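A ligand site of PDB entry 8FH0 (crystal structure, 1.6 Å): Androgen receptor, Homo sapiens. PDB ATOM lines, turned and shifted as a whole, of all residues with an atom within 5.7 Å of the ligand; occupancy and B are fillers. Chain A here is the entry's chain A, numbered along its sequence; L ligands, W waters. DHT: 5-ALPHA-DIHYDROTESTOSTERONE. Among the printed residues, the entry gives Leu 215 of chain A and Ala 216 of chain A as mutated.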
ATOM      1  N   LEU A  40       3.043  -2.516 -28.113  1.00  0.00           N
ATOM      2  CA  LEU A  40       3.311  -1.072 -28.053  1.00  0.00           C
ATOM      3  C   LEU A  40       2.821  -0.470 -26.750  1.00  0.00           C
ATOM      4  O   LEU A  40       3.458   0.436 -26.215  1.00  0.00           O
ATOM      5  CB  LEU A  40       2.695  -0.371 -29.266  1.00  0.00           C
ATOM      6  CG  LEU A  40       3.672  -0.195 -30.419  1.00  0.00           C
ATOM      7  CD1 LEU A  40       4.868   0.690 -30.068  1.00  0.00           C
ATOM      8  CD2 LEU A  40       4.168  -1.544 -30.891  1.00  0.00           C
ATOM      9  N   LEU A  43       5.607  -1.161 -24.337  1.00  0.00           N
ATOM     10  CA  LEU A  43       6.755  -0.295 -24.593  1.00  0.00           C
ATOM     11  C   LEU A  43       6.494   1.112 -24.076  1.00  0.00           C
ATOM     12  O   LEU A  43       7.397   1.743 -23.503  1.00  0.00           O
ATOM     13  CB  LEU A  43       7.097  -0.261 -26.081  1.00  0.00           C
ATOM     14  CG  LEU A  43       7.816  -1.468 -26.668  1.00  0.00           C
ATOM     15  CD1 LEU A  43       7.834  -1.356 -28.177  1.00  0.00           C
ATOM     16  CD2 LEU A  43       9.239  -1.530 -26.174  1.00  0.00           C
ATOM     17  N   ASN A  44       5.266   1.620 -24.248  1.00  0.00           N
ATOM     18  CA  ASN A  44       4.938   2.959 -23.758  1.00  0.00           C
ATOM     19  C   ASN A  44       5.000   3.001 -22.245  1.00  0.00           C
ATOM     20  O   ASN A  44       5.494   3.973 -21.663  1.00  0.00           O
ATOM     21  CB  ASN A  44       3.543   3.386 -24.238  1.00  0.00           C
ATOM     22  CG  ASN A  44       3.495   3.656 -25.713  1.00  0.00           C
ATOM     23  OD1 ASN A  44       4.511   3.933 -26.342  1.00  0.00           O
ATOM     24  ND2 ASN A  44       2.302   3.604 -26.284  1.00  0.00           N
ATOM     25  N   LEU A  46       6.868   1.026 -20.394  1.00  0.00           N
ATOM     26  CA  LEU A  46       8.294   0.984 -20.086  1.00  0.00           C
ATOM     27  C   LEU A  46       8.935   2.368 -20.213  1.00  0.00           C
ATOM     28  O   LEU A  46       9.751   2.760 -19.387  1.00  0.00           O
ATOM     29  CB  LEU A  46       9.006  -0.011 -21.009  1.00  0.00           C
ATOM     30  CG  LEU A  46      10.510  -0.138 -20.750  1.00  0.00           C
ATOM     31  CD1 LEU A  46      10.773  -0.683 -19.317  1.00  0.00           C
ATOM     32  CD2 LEU A  46      11.143  -1.077 -21.769  1.00  0.00           C
ATOM     33  N   GLY A  47       8.603   3.092 -21.288  1.00  0.00           N
ATOM     34  CA  GLY A  47       9.113   4.439 -21.428  1.00  0.00           C
ATOM     35  C   GLY A  47       8.723   5.343 -20.274  1.00  0.00           C
ATOM     36  O   GLY A  47       9.535   6.116 -19.775  1.00  0.00           O
ATOM     37  N   GLN A  50      10.809   4.279 -17.281  1.00  0.00           N
ATOM     38  CA  GLN A  50      12.205   4.634 -17.410  1.00  0.00           C
ATOM     39  C   GLN A  50      12.405   6.152 -17.320  1.00  0.00           C
ATOM     40  O   GLN A  50      13.429   6.607 -16.799  1.00  0.00           O
ATOM     41  CB  GLN A  50      12.773   4.117 -18.741  1.00  0.00           C
ATOM     42  CG  GLN A  50      13.226   2.641 -18.636  1.00  0.00           C
ATOM     43  CD  GLN A  50      13.884   2.120 -19.881  1.00  0.00           C
ATOM     44  OE1 GLN A  50      14.296   2.893 -20.742  1.00  0.00           O
ATOM     45  NE2 GLN A  50      13.932   0.801 -20.021  1.00  0.00           N
ATOM     46  N   TRP A  80      15.843  11.979 -24.111  1.00  0.00           N
ATOM     47  CA  TRP A  80      15.446  10.723 -23.480  1.00  0.00           C
ATOM     48  C   TRP A  80      15.444   9.544 -24.458  1.00  0.00           C
ATOM     49  O   TRP A  80      15.844   8.449 -24.073  1.00  0.00           O
ATOM     50  CB  TRP A  80      14.093  10.858 -22.782  1.00  0.00           C
ATOM     51  CG  TRP A  80      12.945  11.172 -23.694  1.00  0.00           C
ATOM     52  CD1 TRP A  80      12.558  12.406 -24.107  1.00  0.00           C
ATOM     53  CD2 TRP A  80      12.041  10.236 -24.308  1.00  0.00           C
ATOM     54  NE1 TRP A  80      11.468  12.319 -24.935  1.00  0.00           N
ATOM     55  CE2 TRP A  80      11.118  11.003 -25.066  1.00  0.00           C
ATOM     56  CE3 TRP A  80      11.894   8.851 -24.275  1.00  0.00           C
ATOM     57  CZ2 TRP A  80      10.084  10.416 -25.808  1.00  0.00           C
ATOM     58  CZ3 TRP A  80      10.866   8.268 -24.983  1.00  0.00           C
ATOM     59  CH2 TRP A  80       9.976   9.046 -25.752  1.00  0.00           C
ATOM     60  N   MET A  81      14.974   9.731 -25.694  1.00  0.00           N
ATOM     61  CA  MET A  81      14.950   8.608 -26.634  1.00  0.00           C
ATOM     62  C   MET A  81      16.343   8.039 -26.832  1.00  0.00           C
ATOM     63  O   MET A  81      16.564   6.818 -26.776  1.00  0.00           O
ATOM     64  CB  MET A  81      14.439   9.060 -28.004  1.00  0.00           C
ATOM     65  CG  MET A  81      14.110   7.950 -29.005  1.00  0.00           C
ATOM     66  SD  MET A  81      12.986   6.644 -28.437  1.00  0.00           S
ATOM     67  CE  MET A  81      11.438   7.500 -28.770  1.00  0.00           C
ATOM     68  N   MET A  84      17.691   6.230 -23.773  1.00  0.00           N
ATOM     69  CA  MET A  84      16.998   4.980 -23.502  1.00  0.00           C
ATOM     70  C   MET A  84      17.393   3.910 -24.509  1.00  0.00           C
ATOM     71  O   MET A  84      17.527   2.725 -24.167  1.00  0.00           O
ATOM     72  CB  MET A  84      15.508   5.294 -23.560  1.00  0.00           C
ATOM     73  CG  MET A  84      14.981   5.924 -22.278  1.00  0.00           C
ATOM     74  SD  MET A  84      13.193   5.953 -22.246  1.00  0.00           S
ATOM     75  CE  MET A  84      12.973   7.245 -21.014  1.00  0.00           C
ATOM     76  N   VAL A  85      17.598   4.319 -25.763  1.00  0.00           N
ATOM     77  CA  VAL A  85      17.975   3.356 -26.796  1.00  0.00           C
ATOM     78  C   VAL A  85      19.419   2.918 -26.601  1.00  0.00           C
ATOM     79  O   VAL A  85      19.764   1.746 -26.783  1.00  0.00           O
ATOM     80  CB  VAL A  85      17.759   3.965 -28.194  1.00  0.00           C
ATOM     81  CG1 VAL A  85      18.486   3.126 -29.242  1.00  0.00           C
ATOM     82  CG2 VAL A  85      16.274   4.106 -28.513  1.00  0.00           C
ATOM     83  N   MET A  88      19.416   0.546 -23.690  1.00  0.00           N
ATOM     84  CA  MET A  88      18.818  -0.724 -24.065  1.00  0.00           C
ATOM     85  C   MET A  88      19.768  -1.510 -24.952  1.00  0.00           C
ATOM     86  O   MET A  88      19.860  -2.735 -24.853  1.00  0.00           O
ATOM     87  CB  MET A  88      17.489  -0.472 -24.797  1.00  0.00           C
ATOM     88  CG  MET A  88      16.755  -1.736 -25.238  1.00  0.00           C
ATOM     89  SD  MET A  88      17.282  -2.448 -26.795  1.00  0.00           S
ATOM     90  CE  MET A  88      16.628  -1.249 -27.944  1.00  0.00           C
ATOM     91  N   ARG A  91      22.174  -3.205 -22.602  1.00  0.00           N
ATOM     92  CA  ARG A  91      21.501  -4.342 -21.964  1.00  0.00           C
ATOM     93  C   ARG A  91      21.432  -5.522 -22.915  1.00  0.00           C
ATOM     94  O   ARG A  91      21.655  -6.671 -22.530  1.00  0.00           O
ATOM     95  CB  ARG A  91      20.081  -3.937 -21.569  1.00  0.00           C
ATOM     96  CG  ARG A  91      19.951  -3.065 -20.341  1.00  0.00           C
ATOM     97  CD  ARG A  91      18.533  -3.100 -19.772  1.00  0.00           C
ATOM     98  NE  ARG A  91      17.512  -2.565 -20.666  1.00  0.00           N
ATOM     99  CZ  ARG A  91      17.319  -1.280 -20.906  1.00  0.00           C
ATOM    100  NH1 ARG A  91      18.129  -0.344 -20.411  1.00  0.00           N
ATOM    101  NH2 ARG A  91      16.293  -0.916 -21.672  1.00  0.00           N
ATOM    102  N   TYR A 102      16.662  -6.483 -25.632  1.00  0.00           N
ATOM    103  CA  TYR A 102      16.328  -6.615 -24.213  1.00  0.00           C
ATOM    104  C   TYR A 102      15.809  -5.277 -23.689  1.00  0.00           C
ATOM    105  O   TYR A 102      16.473  -4.544 -22.961  1.00  0.00           O
ATOM    106  CB  TYR A 102      17.577  -7.048 -23.449  1.00  0.00           C
ATOM    107  CG  TYR A 102      17.367  -7.610 -22.050  1.00  0.00           C
ATOM    108  CD1 TYR A 102      17.148  -8.956 -21.839  1.00  0.00           C
ATOM    109  CD2 TYR A 102      17.408  -6.768 -20.948  1.00  0.00           C
ATOM    110  CE1 TYR A 102      16.972  -9.466 -20.562  1.00  0.00           C
ATOM    111  CE2 TYR A 102      17.230  -7.257 -19.664  1.00  0.00           C
ATOM    112  CZ  TYR A 102      17.017  -8.612 -19.480  1.00  0.00           C
ATOM    113  OH  TYR A 102      16.836  -9.110 -18.198  1.00  0.00           O
ATOM    114  N   PHE A 103      14.576  -4.955 -24.089  1.00  0.00           N
ATOM    115  CA  PHE A 103      13.967  -3.720 -23.595  1.00  0.00           C
ATOM    116  C   PHE A 103      13.831  -3.779 -22.076  1.00  0.00           C
ATOM    117  O   PHE A 103      14.098  -2.787 -21.382  1.00  0.00           O
ATOM    118  CB  PHE A 103      12.594  -3.499 -24.240  1.00  0.00           C
ATOM    119  CG  PHE A 103      12.659  -3.176 -25.700  1.00  0.00           C
ATOM    120  CD1 PHE A 103      12.994  -1.907 -26.143  1.00  0.00           C
ATOM    121  CD2 PHE A 103      12.354  -4.143 -26.642  1.00  0.00           C
ATOM    122  CE1 PHE A 103      13.053  -1.613 -27.486  1.00  0.00           C
ATOM    123  CE2 PHE A 103      12.399  -3.862 -28.006  1.00  0.00           C
ATOM    124  CZ  PHE A 103      12.745  -2.590 -28.429  1.00  0.00           C
ATOM    125  N   MET A 119       7.726  -2.557 -36.059  1.00  0.00           N
ATOM    126  CA  MET A 119       8.932  -1.751 -35.895  1.00  0.00           C
ATOM    127  C   MET A 119      10.164  -2.503 -36.380  1.00  0.00           C
ATOM    128  O   MET A 119      11.268  -2.263 -35.904  1.00  0.00           O
ATOM    129  CB  MET A 119       9.150  -1.359 -34.424  1.00  0.00           C
ATOM    130  CG  MET A 119       8.103  -0.451 -33.796  1.00  0.00           C
ATOM    131  SD  MET A 119       8.209  -0.520 -31.975  1.00  0.00           S
ATOM    132  CE  MET A 119       9.979  -0.375 -31.796  1.00  0.00           C
ATOM    133  N   MET A 126      18.474  -0.829 -34.197  1.00  0.00           N
ATOM    134  CA  MET A 126      18.751  -0.917 -32.758  1.00  0.00           C
ATOM    135  C   MET A 126      19.647  -2.101 -32.462  1.00  0.00           C
ATOM    136  O   MET A 126      20.561  -2.025 -31.632  1.00  0.00           O
ATOM    137  CB  MET A 126      17.411  -1.035 -32.056  1.00  0.00           C
ATOM    138  CG  MET A 126      16.667   0.295 -32.018  1.00  0.00           C
ATOM    139  SD  MET A 126      15.512   0.549 -30.675  1.00  0.00           S
ATOM    140  CE  MET A 126      14.054  -0.171 -31.429  1.00  0.00           C
ATOM    141  N   LEU A 212      12.608   6.725 -34.222  1.00  0.00           N
ATOM    142  CA  LEU A 212      11.696   6.294 -33.166  1.00  0.00           C
ATOM    143  C   LEU A 212      10.797   7.438 -32.717  1.00  0.00           C
ATOM    144  O   LEU A 212       9.622   7.219 -32.410  1.00  0.00           O
ATOM    145  CB  LEU A 212      12.490   5.730 -31.995  1.00  0.00           C
ATOM    146  CG  LEU A 212      13.257   4.458 -32.363  1.00  0.00           C
ATOM    147  CD1 LEU A 212      14.272   4.134 -31.297  1.00  0.00           C
ATOM    148  CD2 LEU A 212      12.296   3.280 -32.568  1.00  0.00           C
ATOM    149  N   LEU A 215       8.042   7.521 -35.170  1.00  0.00           N
ATOM    150  CA  LEU A 215       7.114   6.437 -34.928  1.00  0.00           C
ATOM    151  C   LEU A 215       6.234   6.735 -33.730  1.00  0.00           C
ATOM    152  O   LEU A 215       5.015   6.551 -33.779  1.00  0.00           O
ATOM    153  CB  LEU A 215       7.897   5.138 -34.724  1.00  0.00           C
ATOM    154  CG  LEU A 215       7.417   3.798 -35.261  1.00  0.00           C
ATOM    155  CD1 LEU A 215       7.188   3.860 -36.773  1.00  0.00           C
ATOM    156  CD2 LEU A 215       8.435   2.715 -34.870  1.00  0.00           C
ATOM    157  N   ALA A 216       6.848   7.233 -32.651  1.00  0.00           N
ATOM    158  CA  ALA A 216       6.108   7.577 -31.451  1.00  0.00           C
ATOM    159  C   ALA A 216       5.036   8.619 -31.742  1.00  0.00           C
ATOM    160  O   ALA A 216       3.903   8.517 -31.257  1.00  0.00           O
ATOM    161  CB  ALA A 216       7.061   8.104 -30.379  1.00  0.00           C
ATOM    162  N   LEU A 219       2.160   7.204 -33.870  1.00  0.00           N
ATOM    163  CA  LEU A 219       1.352   6.275 -33.086  1.00  0.00           C
ATOM    164  C   LEU A 219       0.479   7.023 -32.074  1.00  0.00           C
ATOM    165  O   LEU A 219      -0.680   6.664 -31.864  1.00  0.00           O
ATOM    166  CB  LEU A 219       2.267   5.264 -32.392  1.00  0.00           C
ATOM    167  CG  LEU A 219       1.534   4.171 -31.624  1.00  0.00           C
ATOM    168  CD1 LEU A 219       0.747   3.295 -32.585  1.00  0.00           C
ATOM    169  CD2 LEU A 219       2.555   3.336 -30.861  1.00  0.00           C
ATOM    170  N   PHE A 230      -1.282   5.401 -24.198  1.00  0.00           N
ATOM    171  CA  PHE A 230      -0.112   6.227 -23.889  1.00  0.00           C
ATOM    172  C   PHE A 230      -0.216   6.766 -22.473  1.00  0.00           C
ATOM    173  O   PHE A 230      -1.187   7.462 -22.149  1.00  0.00           O
ATOM    174  CB  PHE A 230       0.030   7.378 -24.877  1.00  0.00           C
ATOM    175  CG  PHE A 230       0.768   7.001 -26.131  1.00  0.00           C
ATOM    176  CD1 PHE A 230       0.101   6.400 -27.189  1.00  0.00           C
ATOM    177  CD2 PHE A 230       2.126   7.227 -26.240  1.00  0.00           C
ATOM    178  CE1 PHE A 230       0.782   6.049 -28.343  1.00  0.00           C
ATOM    179  CE2 PHE A 230       2.822   6.880 -27.389  1.00  0.00           C
ATOM    180  CZ  PHE A 230       2.143   6.284 -28.451  1.00  0.00           C
ATOM    181  N   MET A 234       4.391  10.300 -21.164  1.00  0.00           N
ATOM    182  CA  MET A 234       4.667   9.999 -22.575  1.00  0.00           C
ATOM    183  C   MET A 234       3.765  10.808 -23.498  1.00  0.00           C
ATOM    184  O   MET A 234       4.226  11.371 -24.492  1.00  0.00           O
ATOM    185  CB  MET A 234       4.533   8.503 -22.866  1.00  0.00           C
ATOM    186  CG  MET A 234       5.556   7.539 -22.235  1.00  0.00           C
ATOM    187  SD  MET A 234       7.227   7.797 -22.883  1.00  0.00           S
ATOM    188  CE  MET A 234       7.275   6.530 -24.148  1.00  0.00           C
ATOM    189  N   ILE A 238       5.451  13.534 -26.013  1.00  0.00           N
ATOM    190  CA  ILE A 238       5.421  13.240 -27.441  1.00  0.00           C
ATOM    191  C   ILE A 238       4.602  14.279 -28.189  1.00  0.00           C
ATOM    192  O   ILE A 238       4.840  14.514 -29.376  1.00  0.00           O
ATOM    193  CB  ILE A 238       4.910  11.820 -27.696  1.00  0.00           C
ATOM    194  CG1 ILE A 238       5.942  10.816 -27.162  1.00  0.00           C
ATOM    195  CG2 ILE A 238       4.680  11.576 -29.182  1.00  0.00           C
ATOM    196  CD1 ILE A 238       5.415   9.379 -27.032  1.00  0.00           C
HETATM  197  C1  DHT L   1      11.312   2.216 -24.124  1.00  0.00           C
HETATM  198  C2  DHT L   1      12.595   2.063 -23.307  1.00  0.00           C
HETATM  199  C3  DHT L   1      13.656   1.335 -24.075  1.00  0.00           C
HETATM  200  O3  DHT L   1      14.299   0.425 -23.585  1.00  0.00           O
HETATM  201  C4  DHT L   1      13.855   1.775 -25.496  1.00  0.00           C
HETATM  202  C5  DHT L   1      12.525   1.891 -26.249  1.00  0.00           C
HETATM  203  C6  DHT L   1      12.757   2.424 -27.655  1.00  0.00           C
HETATM  204  C7  DHT L   1      11.441   2.463 -28.428  1.00  0.00           C
HETATM  205  C8  DHT L   1      10.401   3.350 -27.753  1.00  0.00           C
HETATM  206  C9  DHT L   1      10.203   2.874 -26.310  1.00  0.00           C
HETATM  207  C10 DHT L   1      11.542   2.833 -25.513  1.00  0.00           C
HETATM  208  C11 DHT L   1       9.146   3.729 -25.604  1.00  0.00           C
HETATM  209  C12 DHT L   1       7.816   3.728 -26.361  1.00  0.00           C
HETATM  210  C13 DHT L   1       7.991   4.130 -27.831  1.00  0.00           C
HETATM  211  C14 DHT L   1       9.051   3.204 -28.447  1.00  0.00           C
HETATM  212  C15 DHT L   1       8.964   3.565 -29.933  1.00  0.00           C
HETATM  213  C16 DHT L   1       7.463   3.846 -30.155  1.00  0.00           C
HETATM  214  C17 DHT L   1       6.818   3.799 -28.759  1.00  0.00           C
HETATM  215  O17 DHT L   1       5.795   4.796 -28.701  1.00  0.00           O
HETATM  216  C18 DHT L   1       8.353   5.622 -27.931  1.00  0.00           C
HETATM  217  C19 DHT L   1      12.120   4.243 -25.345  1.00  0.00           C
HETATM  218  O   HOH W   1      16.673   1.987 -21.686  1.00  0.00           O
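Leu 40 touches the ligand (CD1 to C17, 3.9 Å). Leu 43 touches the ligand. CD2 of Leu 46 touches C2 of the ligand (3.8 Å). OE1 of Gln 50 touches C2 of the ligand, 3.2 Å away. Met 81 touches the ligand (CE to C18, 3.7 Å). SD of Met 84 touches C19 of the ligand (3.7 Å). Val 85 touches the ligand. Met 88 touches the ligand (CB to O3, 3.5 Å). Phe 103 touches the ligand (CD1 to O3, 3.7 Å). Ala 216 touches the ligand. CE2 of Phe 230 touches O17 of the ligand, 3.9 Å away. Met 234 touches the ligand. Hydrophobic or aromatic side chains that line the ligand: Leu 40, Leu 46, Met 81, Met 84, Val 85, Met 88, Phe 103, Ala 216, Phe 230 and Met 234. Of the 23 residues printed, 14 come within 4 Å of the ligand.
O of Leu 40 sits close to ND2 of Asn 44, at 3.4 Å. NH2 of Arg 91 sits close to NE2 of Gln 50 (3.4 Å). NH2 of Arg 91 is in hydrogen-bond range of O of Phe 103, at 2.9 Å. NE of Arg 91 sits at hydrogen-bond distance from O of Tyr 102, at 3.2 Å. OE1 of Gln 50 sits close to SD of Met 84 (3.6 Å).
OD1 of Asn 44 is in hydrogen-bond range of O17 of the ligand (2.8 Å). An oxygen (O3) of the ligand sits at hydrogen-bond distance from the guanidinium group (NH2) of Arg 91 (3.1 Å).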
